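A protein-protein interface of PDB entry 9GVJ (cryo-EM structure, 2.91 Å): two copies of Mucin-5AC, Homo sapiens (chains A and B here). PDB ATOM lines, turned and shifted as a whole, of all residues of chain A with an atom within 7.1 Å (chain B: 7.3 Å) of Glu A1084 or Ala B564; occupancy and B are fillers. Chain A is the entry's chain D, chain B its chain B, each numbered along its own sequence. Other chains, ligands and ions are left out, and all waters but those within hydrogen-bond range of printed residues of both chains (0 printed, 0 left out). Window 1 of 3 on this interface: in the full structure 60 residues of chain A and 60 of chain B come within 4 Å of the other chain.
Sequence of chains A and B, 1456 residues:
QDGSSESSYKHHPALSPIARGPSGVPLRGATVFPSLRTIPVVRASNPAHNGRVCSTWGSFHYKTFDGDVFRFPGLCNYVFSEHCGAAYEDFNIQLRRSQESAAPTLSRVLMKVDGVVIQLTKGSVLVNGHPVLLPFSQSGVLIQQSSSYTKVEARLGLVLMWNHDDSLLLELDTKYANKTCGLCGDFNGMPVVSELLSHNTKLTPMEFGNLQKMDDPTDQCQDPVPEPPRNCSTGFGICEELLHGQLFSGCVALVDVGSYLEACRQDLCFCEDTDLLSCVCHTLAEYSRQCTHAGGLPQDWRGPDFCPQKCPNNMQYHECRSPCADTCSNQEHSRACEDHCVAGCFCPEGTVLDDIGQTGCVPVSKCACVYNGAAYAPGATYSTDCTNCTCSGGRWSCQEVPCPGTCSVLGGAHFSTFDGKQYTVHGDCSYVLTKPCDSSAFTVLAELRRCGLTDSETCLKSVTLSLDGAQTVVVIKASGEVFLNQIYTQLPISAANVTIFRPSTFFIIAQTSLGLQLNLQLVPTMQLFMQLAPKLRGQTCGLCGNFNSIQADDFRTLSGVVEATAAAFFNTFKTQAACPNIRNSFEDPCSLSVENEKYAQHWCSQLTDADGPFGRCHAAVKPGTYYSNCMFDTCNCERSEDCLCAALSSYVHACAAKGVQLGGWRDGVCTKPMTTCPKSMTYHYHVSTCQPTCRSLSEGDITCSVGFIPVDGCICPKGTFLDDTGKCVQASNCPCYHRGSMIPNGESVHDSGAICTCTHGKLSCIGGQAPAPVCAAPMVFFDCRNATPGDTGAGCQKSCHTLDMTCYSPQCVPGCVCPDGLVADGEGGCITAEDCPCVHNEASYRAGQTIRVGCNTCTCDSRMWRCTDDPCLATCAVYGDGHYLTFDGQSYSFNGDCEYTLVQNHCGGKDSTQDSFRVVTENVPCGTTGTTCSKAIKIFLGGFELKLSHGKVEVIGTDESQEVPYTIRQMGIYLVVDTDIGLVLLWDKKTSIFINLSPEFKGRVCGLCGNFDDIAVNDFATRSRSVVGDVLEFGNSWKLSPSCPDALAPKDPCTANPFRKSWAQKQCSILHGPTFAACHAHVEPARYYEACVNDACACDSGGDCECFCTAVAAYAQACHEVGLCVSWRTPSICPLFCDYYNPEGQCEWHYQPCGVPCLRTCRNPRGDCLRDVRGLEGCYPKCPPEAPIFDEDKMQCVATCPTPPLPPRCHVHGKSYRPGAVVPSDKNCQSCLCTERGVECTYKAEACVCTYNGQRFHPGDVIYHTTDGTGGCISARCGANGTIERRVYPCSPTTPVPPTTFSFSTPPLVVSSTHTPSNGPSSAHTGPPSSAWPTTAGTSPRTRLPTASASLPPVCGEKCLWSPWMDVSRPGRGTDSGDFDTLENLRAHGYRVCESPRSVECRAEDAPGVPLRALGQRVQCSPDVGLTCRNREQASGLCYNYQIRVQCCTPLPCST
Of the printed residues of chain B, His A1080 touches Thr B565 and Phe B586. Of the printed residues of chain B, His A1082 touches Ala B564 (3.1 Å). Of the printed residues of chain B, Glu A1084 touches Ala B564 (3.7 Å) and Ala B566 (3.5 Å). Printed residues of chain B within 4 Å of Pro A1085: Phe B586 (3.7 Å). Ala B564 touches just these residues of chain A: Asn A841, Ala A1081, His A1082 and Glu A1084. Printed residues of chain A within 4 Å of Thr B565: His A1080. The nearest printed residue of chain B that does not touch Glu A1084 is Thr B565 (4.01 Å). The nearest printed residue of chain B that does not touch His A1080 is Ala B564 (6.3 Å).
Printed residues of chain B that touch a printed residue of chain A: Val B562, Glu B563, Ala B564, Thr B565, Ala B566 and Phe B586. Printed residues of chain A that touch a printed residue of chain B: His A840, Asn A841, His A1080, Ala A1081, His A1082, Glu A1084 and Pro A1085. Among the printed residues, no Asp or Glu carboxylate lies within 4 Å of a Lys or Arg side-chain nitrogen of the other chain.
No position is printed for both chains. Of the 11 pairs that touch across the chains among the printed residues, none has its exchanged pair printed and touching as well.
A ring nitrogen (ND1) of His A840 is in hydrogen-bond range of the side-chain carboxylate (OE1) of Glu B563 (2.8 Å). The side-chain amide oxygen of Asn A841 lies within hydrogen-bond range of the backbone NH of Ala B564, 3.1 Å away.
Among the printed residues, merely in contact across the chains: His A840 with Val B562, Asn A841 with Glu B563, His A1080 with Thr B565, His A1080 with Phe B586, Ala A1081 with Ala B564, His A1082 with Ala B564, Glu A1084 with Ala B564, Glu A1084 with Ala B566 and Pro A1085 with Phe B586.
The backbone NH (N) of Glu B563 sits at hydrogen-bond distance from the backbone carbonyl oxygen (O) of Phe B555 (2.9 Å). A ring nitrogen (NE2) of His A840 is in hydrogen-bond range of the side-chain amide nitrogen (ND2) of Asn A841 (3.3 Å).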
ATOM      1  N   HIS A 840      -8.457  23.771 -11.864  1.00  0.00           N
ATOM      2  CA  HIS A 840      -8.060  22.692 -12.758  1.00  0.00           C
ATOM      3  C   HIS A 840      -7.154  21.724 -12.012  1.00  0.00           C
ATOM      4  O   HIS A 840      -6.157  22.142 -11.418  1.00  0.00           O
ATOM      5  CB  HIS A 840      -7.342  23.234 -13.999  1.00  0.00           C
ATOM      6  CG  HIS A 840      -7.132  22.208 -15.069  1.00  0.00           C
ATOM      7  ND1 HIS A 840      -8.156  21.435 -15.572  1.00  0.00           N
ATOM      8  CD2 HIS A 840      -6.013  21.825 -15.729  1.00  0.00           C
ATOM      9  CE1 HIS A 840      -7.678  20.623 -16.497  1.00  0.00           C
ATOM     10  NE2 HIS A 840      -6.380  20.839 -16.612  1.00  0.00           N
ATOM     11  N   ASN A 841      -7.512  20.440 -12.051  1.00  0.00           N
ATOM     12  CA  ASN A 841      -6.690  19.357 -11.508  1.00  0.00           C
ATOM     13  C   ASN A 841      -6.244  19.652 -10.077  1.00  0.00           C
ATOM     14  O   ASN A 841      -5.057  19.605  -9.746  1.00  0.00           O
ATOM     15  CB  ASN A 841      -5.486  19.084 -12.411  1.00  0.00           C
ATOM     16  CG  ASN A 841      -5.868  18.356 -13.683  1.00  0.00           C
ATOM     17  OD1 ASN A 841      -6.901  17.690 -13.745  1.00  0.00           O
ATOM     18  ND2 ASN A 841      -5.032  18.477 -14.708  1.00  0.00           N
ATOM     19  N   CYS A1079       1.755  13.444  -9.233  1.00  0.00           N
ATOM     20  CA  CYS A1079       1.099  13.007 -10.457  1.00  0.00           C
ATOM     21  C   CYS A1079      -0.322  12.511 -10.227  1.00  0.00           C
ATOM     22  O   CYS A1079      -1.097  12.425 -11.186  1.00  0.00           O
ATOM     23  CB  CYS A1079       1.923  11.903 -11.122  1.00  0.00           C
ATOM     24  SG  CYS A1079       1.313  11.379 -12.734  1.00  0.00           S
ATOM     25  N   HIS A1080      -0.688  12.199  -8.981  1.00  0.00           N
ATOM     26  CA  HIS A1080      -1.996  11.616  -8.708  1.00  0.00           C
ATOM     27  C   HIS A1080      -3.142  12.539  -9.101  1.00  0.00           C
ATOM     28  O   HIS A1080      -4.248  12.057  -9.365  1.00  0.00           O
ATOM     29  CB  HIS A1080      -2.103  11.249  -7.228  1.00  0.00           C
ATOM     30  CG  HIS A1080      -1.340  10.015  -6.857  1.00  0.00           C
ATOM     31  ND1 HIS A1080      -0.938   9.749  -5.567  1.00  0.00           N
ATOM     32  CD2 HIS A1080      -0.904   8.977  -7.610  1.00  0.00           C
ATOM     33  CE1 HIS A1080      -0.288   8.598  -5.539  1.00  0.00           C
ATOM     34  NE2 HIS A1080      -0.253   8.111  -6.766  1.00  0.00           N
ATOM     35  N   ALA A1081      -2.907  13.850  -9.145  1.00  0.00           N
ATOM     36  CA  ALA A1081      -3.933  14.791  -9.567  1.00  0.00           C
ATOM     37  C   ALA A1081      -4.006  14.956 -11.079  1.00  0.00           C
ATOM     38  O   ALA A1081      -4.930  15.613 -11.567  1.00  0.00           O
ATOM     39  CB  ALA A1081      -3.697  16.155  -8.914  1.00  0.00           C
ATOM     40  N   HIS A1082      -3.062  14.383 -11.828  1.00  0.00           N
ATOM     41  CA  HIS A1082      -3.023  14.539 -13.275  1.00  0.00           C
ATOM     42  C   HIS A1082      -3.112  13.234 -14.051  1.00  0.00           C
ATOM     43  O   HIS A1082      -3.504  13.266 -15.223  1.00  0.00           O
ATOM     44  CB  HIS A1082      -1.744  15.277 -13.702  1.00  0.00           C
ATOM     45  CG  HIS A1082      -1.492  16.540 -12.939  1.00  0.00           C
ATOM     46  ND1 HIS A1082      -1.789  17.787 -13.445  1.00  0.00           N
ATOM     47  CD2 HIS A1082      -0.966  16.749 -11.708  1.00  0.00           C
ATOM     48  CE1 HIS A1082      -1.460  18.709 -12.558  1.00  0.00           C
ATOM     49  NE2 HIS A1082      -0.958  18.106 -11.497  1.00  0.00           N
ATOM     50  N   VAL A1083      -2.737  12.103 -13.460  1.00  0.00           N
ATOM     51  CA  VAL A1083      -2.909  10.793 -14.080  1.00  0.00           C
ATOM     52  C   VAL A1083      -3.481   9.852 -13.030  1.00  0.00           C
ATOM     53  O   VAL A1083      -2.915   9.721 -11.938  1.00  0.00           O
ATOM     54  CB  VAL A1083      -1.594  10.232 -14.648  1.00  0.00           C
ATOM     55  CG1 VAL A1083      -1.858   8.940 -15.402  1.00  0.00           C
ATOM     56  CG2 VAL A1083      -0.920  11.243 -15.563  1.00  0.00           C
ATOM     57  N   GLU A1084      -4.593   9.206 -13.352  1.00  0.00           N
ATOM     58  CA  GLU A1084      -5.223   8.284 -12.414  1.00  0.00           C
ATOM     59  C   GLU A1084      -4.423   6.991 -12.340  1.00  0.00           C
ATOM     60  O   GLU A1084      -4.211   6.344 -13.374  1.00  0.00           O
ATOM     61  CB  GLU A1084      -6.662   8.002 -12.835  1.00  0.00           C
ATOM     62  CG  GLU A1084      -7.641   7.942 -11.675  1.00  0.00           C
ATOM     63  CD  GLU A1084      -9.029   8.416 -12.059  1.00  0.00           C
ATOM     64  OE1 GLU A1084      -9.318   8.491 -13.271  1.00  0.00           O
ATOM     65  OE2 GLU A1084      -9.828   8.718 -11.149  1.00  0.00           O
ATOM     66  N   PRO A1085      -3.964   6.575 -11.158  1.00  0.00           N
ATOM     67  CA  PRO A1085      -3.098   5.393 -11.074  1.00  0.00           C
ATOM     68  C   PRO A1085      -3.852   4.090 -10.861  1.00  0.00           C
ATOM     69  O   PRO A1085      -3.244   3.082 -10.490  1.00  0.00           O
ATOM     70  CB  PRO A1085      -2.207   5.715  -9.871  1.00  0.00           C
ATOM     71  CG  PRO A1085      -3.090   6.531  -8.982  1.00  0.00           C
ATOM     72  CD  PRO A1085      -4.067   7.276  -9.867  1.00  0.00           C
ATOM     73  N   ALA A1086      -5.167   4.091 -11.085  1.00  0.00           N
ATOM     74  CA  ALA A1086      -5.975   2.912 -10.780  1.00  0.00           C
ATOM     75  C   ALA A1086      -5.641   1.749 -11.708  1.00  0.00           C
ATOM     76  O   ALA A1086      -5.219   0.676 -11.256  1.00  0.00           O
ATOM     77  CB  ALA A1086      -7.461   3.263 -10.868  1.00  0.00           C
ATOM     78  N   ARG A1087      -5.828   1.942 -13.017  1.00  0.00           N
ATOM     79  CA  ARG A1087      -5.566   0.859 -13.957  1.00  0.00           C
ATOM     80  C   ARG A1087      -4.085   0.503 -14.000  1.00  0.00           C
ATOM     81  O   ARG A1087      -3.738  -0.665 -14.199  1.00  0.00           O
ATOM     82  CB  ARG A1087      -6.078   1.234 -15.351  1.00  0.00           C
ATOM     83  CG  ARG A1087      -5.001   1.601 -16.359  1.00  0.00           C
ATOM     84  CD  ARG A1087      -5.600   2.140 -17.646  1.00  0.00           C
ATOM     85  NE  ARG A1087      -4.723   3.115 -18.284  1.00  0.00           N
ATOM     86  CZ  ARG A1087      -5.070   4.362 -18.573  1.00  0.00           C
ATOM     87  NH1 ARG A1087      -6.278   4.825 -18.295  1.00  0.00           N
ATOM     88  NH2 ARG A1087      -4.183   5.164 -19.153  1.00  0.00           N
ATOM     89  N   TYR A1088      -3.202   1.486 -13.807  1.00  0.00           N
ATOM     90  CA  TYR A1088      -1.774   1.191 -13.776  1.00  0.00           C
ATOM     91  C   TYR A1088      -1.419   0.323 -12.577  1.00  0.00           C
ATOM     92  O   TYR A1088      -0.636  -0.625 -12.703  1.00  0.00           O
ATOM     93  CB  TYR A1088      -0.969   2.489 -13.767  1.00  0.00           C
ATOM     94  CG  TYR A1088      -1.114   3.293 -15.038  1.00  0.00           C
ATOM     95  CD1 TYR A1088      -0.320   3.027 -16.143  1.00  0.00           C
ATOM     96  CD2 TYR A1088      -2.047   4.315 -15.134  1.00  0.00           C
ATOM     97  CE1 TYR A1088      -0.450   3.758 -17.309  1.00  0.00           C
ATOM     98  CE2 TYR A1088      -2.183   5.051 -16.294  1.00  0.00           C
ATOM     99  CZ  TYR A1088      -1.383   4.768 -17.377  1.00  0.00           C
ATOM    100  OH  TYR A1088      -1.518   5.501 -18.534  1.00  0.00           O
ATOM    101  N   TYR A1089      -1.995   0.619 -11.409  1.00  0.00           N
ATOM    102  CA  TYR A1089      -1.765  -0.221 -10.238  1.00  0.00           C
ATOM    103  C   TYR A1089      -2.323  -1.624 -10.445  1.00  0.00           C
ATOM    104  O   TYR A1089      -1.686  -2.616 -10.066  1.00  0.00           O
ATOM    105  CB  TYR A1089      -2.385   0.424  -8.998  1.00  0.00           C
ATOM    106  CG  TYR A1089      -2.383  -0.464  -7.775  1.00  0.00           C
ATOM    107  CD1 TYR A1089      -1.215  -0.698  -7.066  1.00  0.00           C
ATOM    108  CD2 TYR A1089      -3.551  -1.064  -7.328  1.00  0.00           C
ATOM    109  CE1 TYR A1089      -1.209  -1.507  -5.946  1.00  0.00           C
ATOM    110  CE2 TYR A1089      -3.554  -1.876  -6.209  1.00  0.00           C
ATOM    111  CZ  TYR A1089      -2.380  -2.094  -5.523  1.00  0.00           C
ATOM    112  OH  TYR A1089      -2.378  -2.900  -4.409  1.00  0.00           O
ATOM    113  N   TYR A1115       3.188   4.104 -16.050  1.00  0.00           N
ATOM    114  CA  TYR A1115       2.635   5.230 -15.303  1.00  0.00           C
ATOM    115  C   TYR A1115       3.609   6.400 -15.268  1.00  0.00           C
ATOM    116  O   TYR A1115       3.192   7.562 -15.307  1.00  0.00           O
ATOM    117  CB  TYR A1115       2.272   4.795 -13.885  1.00  0.00           C
ATOM    118  CG  TYR A1115       1.531   5.847 -13.091  1.00  0.00           C
ATOM    119  CD1 TYR A1115       0.248   6.234 -13.443  1.00  0.00           C
ATOM    120  CD2 TYR A1115       2.118   6.456 -11.990  1.00  0.00           C
ATOM    121  CE1 TYR A1115      -0.432   7.193 -12.722  1.00  0.00           C
ATOM    122  CE2 TYR A1115       1.446   7.416 -11.263  1.00  0.00           C
ATOM    123  CZ  TYR A1115       0.172   7.780 -11.634  1.00  0.00           C
ATOM    124  OH  TYR A1115      -0.500   8.738 -10.911  1.00  0.00           O
ATOM    125  N   ALA A1118       3.277   8.153 -18.522  1.00  0.00           N
ATOM    126  CA  ALA A1118       2.026   8.906 -18.520  1.00  0.00           C
ATOM    127  C   ALA A1118       2.159  10.193 -17.714  1.00  0.00           C
ATOM    128  O   ALA A1118       1.634  11.240 -18.109  1.00  0.00           O
ATOM    129  CB  ALA A1118       0.893   8.040 -17.969  1.00  0.00           C
ATOM    130  N   LYS B 421     -18.959   6.138 -19.332  1.00  0.00           N
ATOM    131  CA  LYS B 421     -17.859   6.394 -18.413  1.00  0.00           C
ATOM    132  C   LYS B 421     -18.284   6.056 -16.991  1.00  0.00           C
ATOM    133  O   LYS B 421     -19.377   6.428 -16.553  1.00  0.00           O
ATOM    134  CB  LYS B 421     -17.414   7.852 -18.504  1.00  0.00           C
ATOM    135  CG  LYS B 421     -16.172   8.166 -17.691  1.00  0.00           C
ATOM    136  CD  LYS B 421     -15.688   9.581 -17.937  1.00  0.00           C
ATOM    137  CE  LYS B 421     -14.198   9.608 -18.223  1.00  0.00           C
ATOM    138  NZ  LYS B 421     -13.486   8.483 -17.557  1.00  0.00           N
ATOM    139  N   GLN B 422     -17.419   5.351 -16.268  1.00  0.00           N
ATOM    140  CA  GLN B 422     -17.724   4.863 -14.931  1.00  0.00           C
ATOM    141  C   GLN B 422     -16.666   5.349 -13.955  1.00  0.00           C
ATOM    142  O   GLN B 422     -15.466   5.237 -14.227  1.00  0.00           O
ATOM    143  CB  GLN B 422     -17.805   3.336 -14.916  1.00  0.00           C
ATOM    144  CG  GLN B 422     -18.911   2.775 -15.791  1.00  0.00           C
ATOM    145  CD  GLN B 422     -18.914   1.264 -15.825  1.00  0.00           C
ATOM    146  OE1 GLN B 422     -17.896   0.625 -15.562  1.00  0.00           O
ATOM    147  NE2 GLN B 422     -20.060   0.680 -16.150  1.00  0.00           N
ATOM    148  N   TYR B 423     -17.113   5.886 -12.823  1.00  0.00           N
ATOM    149  CA  TYR B 423     -16.209   6.370 -11.790  1.00  0.00           C
ATOM    150  C   TYR B 423     -16.854   6.151 -10.428  1.00  0.00           C
ATOM    151  O   TYR B 423     -17.987   5.673 -10.323  1.00  0.00           O
ATOM    152  CB  TYR B 423     -15.839   7.840 -12.022  1.00  0.00           C
ATOM    153  CG  TYR B 423     -17.015   8.788 -12.106  1.00  0.00           C
ATOM    154  CD1 TYR B 423     -17.734   8.936 -13.284  1.00  0.00           C
ATOM    155  CD2 TYR B 423     -17.395   9.548 -11.011  1.00  0.00           C
ATOM    156  CE1 TYR B 423     -18.805   9.805 -13.364  1.00  0.00           C
ATOM    157  CE2 TYR B 423     -18.462  10.421 -11.081  1.00  0.00           C
ATOM    158  CZ  TYR B 423     -19.162  10.546 -12.258  1.00  0.00           C
ATOM    159  OH  TYR B 423     -20.227  11.414 -12.329  1.00  0.00           O
ATOM    160  N   THR B 424     -16.116   6.497  -9.375  1.00  0.00           N
ATOM    161  CA  THR B 424     -16.582   6.281  -8.008  1.00  0.00           C
ATOM    162  C   THR B 424     -16.046   7.408  -7.137  1.00  0.00           C
ATOM    163  O   THR B 424     -14.847   7.450  -6.847  1.00  0.00           O
ATOM    164  CB  THR B 424     -16.131   4.921  -7.480  1.00  0.00           C
ATOM    165  OG1 THR B 424     -16.723   3.880  -8.266  1.00  0.00           O
ATOM    166  CG2 THR B 424     -16.546   4.749  -6.027  1.00  0.00           C
ATOM    167  N   VAL B 425     -16.928   8.316  -6.728  1.00  0.00           N
ATOM    168  CA  VAL B 425     -16.578   9.418  -5.842  1.00  0.00           C
ATOM    169  C   VAL B 425     -17.540   9.411  -4.664  1.00  0.00           C
ATOM    170  O   VAL B 425     -18.739   9.157  -4.830  1.00  0.00           O
ATOM    171  CB  VAL B 425     -16.619  10.782  -6.563  1.00  0.00           C
ATOM    172  CG1 VAL B 425     -15.851  11.819  -5.765  1.00  0.00           C
ATOM    173  CG2 VAL B 425     -16.049  10.666  -7.963  1.00  0.00           C
ATOM    174  N   PHE B 555     -15.583  14.226 -18.368  1.00  0.00           N
ATOM    175  CA  PHE B 555     -15.004  14.886 -17.206  1.00  0.00           C
ATOM    176  C   PHE B 555     -14.733  16.363 -17.453  1.00  0.00           C
ATOM    177  O   PHE B 555     -13.889  16.954 -16.769  1.00  0.00           O
ATOM    178  CB  PHE B 555     -13.717  14.178 -16.782  1.00  0.00           C
ATOM    179  CG  PHE B 555     -13.944  12.984 -15.904  1.00  0.00           C
ATOM    180  CD1 PHE B 555     -15.228  12.592 -15.568  1.00  0.00           C
ATOM    181  CD2 PHE B 555     -12.875  12.256 -15.413  1.00  0.00           C
ATOM    182  CE1 PHE B 555     -15.442  11.494 -14.761  1.00  0.00           C
ATOM    183  CE2 PHE B 555     -13.082  11.158 -14.606  1.00  0.00           C
ATOM    184  CZ  PHE B 555     -14.368  10.777 -14.279  1.00  0.00           C
ATOM    185  N   VAL B 562     -11.110  19.521 -19.415  1.00  0.00           N
ATOM    186  CA  VAL B 562     -11.375  18.152 -18.986  1.00  0.00           C
ATOM    187  C   VAL B 562     -10.438  17.826 -17.832  1.00  0.00           C
ATOM    188  O   VAL B 562      -9.212  17.890 -17.982  1.00  0.00           O
ATOM    189  CB  VAL B 562     -11.190  17.158 -20.143  1.00  0.00           C
ATOM    190  CG1 VAL B 562     -11.272  15.729 -19.632  1.00  0.00           C
ATOM    191  CG2 VAL B 562     -12.223  17.405 -21.230  1.00  0.00           C
ATOM    192  N   GLU B 563     -11.009  17.479 -16.683  1.00  0.00           N
ATOM    193  CA  GLU B 563     -10.197  17.097 -15.540  1.00  0.00           C
ATOM    194  C   GLU B 563      -9.623  15.697 -15.735  1.00  0.00           C
ATOM    195  O   GLU B 563     -10.087  14.910 -16.564  1.00  0.00           O
ATOM    196  CB  GLU B 563     -11.015  17.151 -14.251  1.00  0.00           C
ATOM    197  CG  GLU B 563     -11.888  18.381 -14.122  1.00  0.00           C
ATOM    198  CD  GLU B 563     -11.124  19.590 -13.621  1.00  0.00           C
ATOM    199  OE1 GLU B 563     -10.406  20.221 -14.425  1.00  0.00           O
ATOM    200  OE2 GLU B 563     -11.243  19.911 -12.420  1.00  0.00           O
ATOM    201  N   ALA B 564      -8.592  15.394 -14.948  1.00  0.00           N
ATOM    202  CA  ALA B 564      -7.912  14.110 -15.035  1.00  0.00           C
ATOM    203  C   ALA B 564      -8.411  13.091 -14.023  1.00  0.00           C
ATOM    204  O   ALA B 564      -8.235  11.888 -14.243  1.00  0.00           O
ATOM    205  CB  ALA B 564      -6.404  14.298 -14.850  1.00  0.00           C
ATOM    206  N   THR B 565      -9.023  13.535 -12.930  1.00  0.00           N
ATOM    207  CA  THR B 565      -9.506  12.647 -11.886  1.00  0.00           C
ATOM    208  C   THR B 565     -11.008  12.820 -11.713  1.00  0.00           C
ATOM    209  O   THR B 565     -11.578  13.868 -12.027  1.00  0.00           O
ATOM    210  CB  THR B 565      -8.795  12.910 -10.552  1.00  0.00           C
ATOM    211  OG1 THR B 565      -8.656  14.322 -10.352  1.00  0.00           O
ATOM    212  CG2 THR B 565      -7.418  12.263 -10.545  1.00  0.00           C
ATOM    213  N   ALA B 566     -11.647  11.763 -11.211  1.00  0.00           N
ATOM    214  CA  ALA B 566     -13.090  11.806 -11.002  1.00  0.00           C
ATOM    215  C   ALA B 566     -13.461  12.785  -9.896  1.00  0.00           C
ATOM    216  O   ALA B 566     -14.502  13.445  -9.971  1.00  0.00           O
ATOM    217  CB  ALA B 566     -13.613  10.407 -10.680  1.00  0.00           C
ATOM    218  N   ALA B 567     -12.625  12.888  -8.859  1.00  0.00           N
ATOM    219  CA  ALA B 567     -12.938  13.765  -7.735  1.00  0.00           C
ATOM    220  C   ALA B 567     -12.900  15.234  -8.139  1.00  0.00           C
ATOM    221  O   ALA B 567     -13.741  16.026  -7.699  1.00  0.00           O
ATOM    222  CB  ALA B 567     -11.972  13.501  -6.581  1.00  0.00           C
ATOM    223  N   ALA B 568     -11.920  15.623  -8.961  1.00  0.00           N
ATOM    224  CA  ALA B 568     -11.804  17.021  -9.362  1.00  0.00           C
ATOM    225  C   ALA B 568     -13.016  17.469 -10.170  1.00  0.00           C
ATOM    226  O   ALA B 568     -13.553  18.559  -9.945  1.00  0.00           O
ATOM    227  CB  ALA B 568     -10.517  17.233 -10.159  1.00  0.00           C
ATOM    228  N   PHE B 569     -13.460  16.639 -11.116  1.00  0.00           N
ATOM    229  CA  PHE B 569     -14.663  16.954 -11.880  1.00  0.00           C
ATOM    230  C   PHE B 569     -15.911  16.871 -11.011  1.00  0.00           C
ATOM    231  O   PHE B 569     -16.860  17.637 -11.212  1.00  0.00           O
ATOM    232  CB  PHE B 569     -14.767  16.012 -13.081  1.00  0.00           C
ATOM    233  CG  PHE B 569     -16.165  15.823 -13.596  1.00  0.00           C
ATOM    234  CD1 PHE B 569     -16.747  16.770 -14.419  1.00  0.00           C
ATOM    235  CD2 PHE B 569     -16.889  14.687 -13.274  1.00  0.00           C
ATOM    236  CE1 PHE B 569     -18.024  16.595 -14.900  1.00  0.00           C
ATOM    237  CE2 PHE B 569     -18.169  14.509 -13.751  1.00  0.00           C
ATOM    238  CZ  PHE B 569     -18.737  15.465 -14.565  1.00  0.00           C
ATOM    239  N   ASN B 584      -9.999  11.901  -3.816  1.00  0.00           N
ATOM    240  CA  ASN B 584     -10.050  10.456  -3.978  1.00  0.00           C
ATOM    241  C   ASN B 584      -8.805   9.810  -3.387  1.00  0.00           C
ATOM    242  O   ASN B 584      -7.679  10.231  -3.673  1.00  0.00           O
ATOM    243  CB  ASN B 584     -10.189  10.088  -5.454  1.00  0.00           C
ATOM    244  CG  ASN B 584     -11.532   9.461  -5.775  1.00  0.00           C
ATOM    245  OD1 ASN B 584     -12.266   9.047  -4.878  1.00  0.00           O
ATOM    246  ND2 ASN B 584     -11.859   9.388  -7.060  1.00  0.00           N
ATOM    247  N   PHE B 586      -6.756   5.988  -2.413  1.00  0.00           N
ATOM    248  CA  PHE B 586      -6.582   4.620  -2.902  1.00  0.00           C
ATOM    249  C   PHE B 586      -6.760   3.618  -1.759  1.00  0.00           C
ATOM    250  O   PHE B 586      -5.849   2.887  -1.373  1.00  0.00           O
ATOM    251  CB  PHE B 586      -5.220   4.472  -3.567  1.00  0.00           C
ATOM    252  CG  PHE B 586      -4.680   5.755  -4.124  1.00  0.00           C
ATOM    253  CD1 PHE B 586      -5.194   6.288  -5.293  1.00  0.00           C
ATOM    254  CD2 PHE B 586      -3.661   6.432  -3.475  1.00  0.00           C
ATOM    255  CE1 PHE B 586      -4.701   7.469  -5.806  1.00  0.00           C
ATOM    256  CE2 PHE B 586      -3.165   7.613  -3.983  1.00  0.00           C
ATOM    257  CZ  PHE B 586      -3.686   8.133  -5.151  1.00  0.00           C
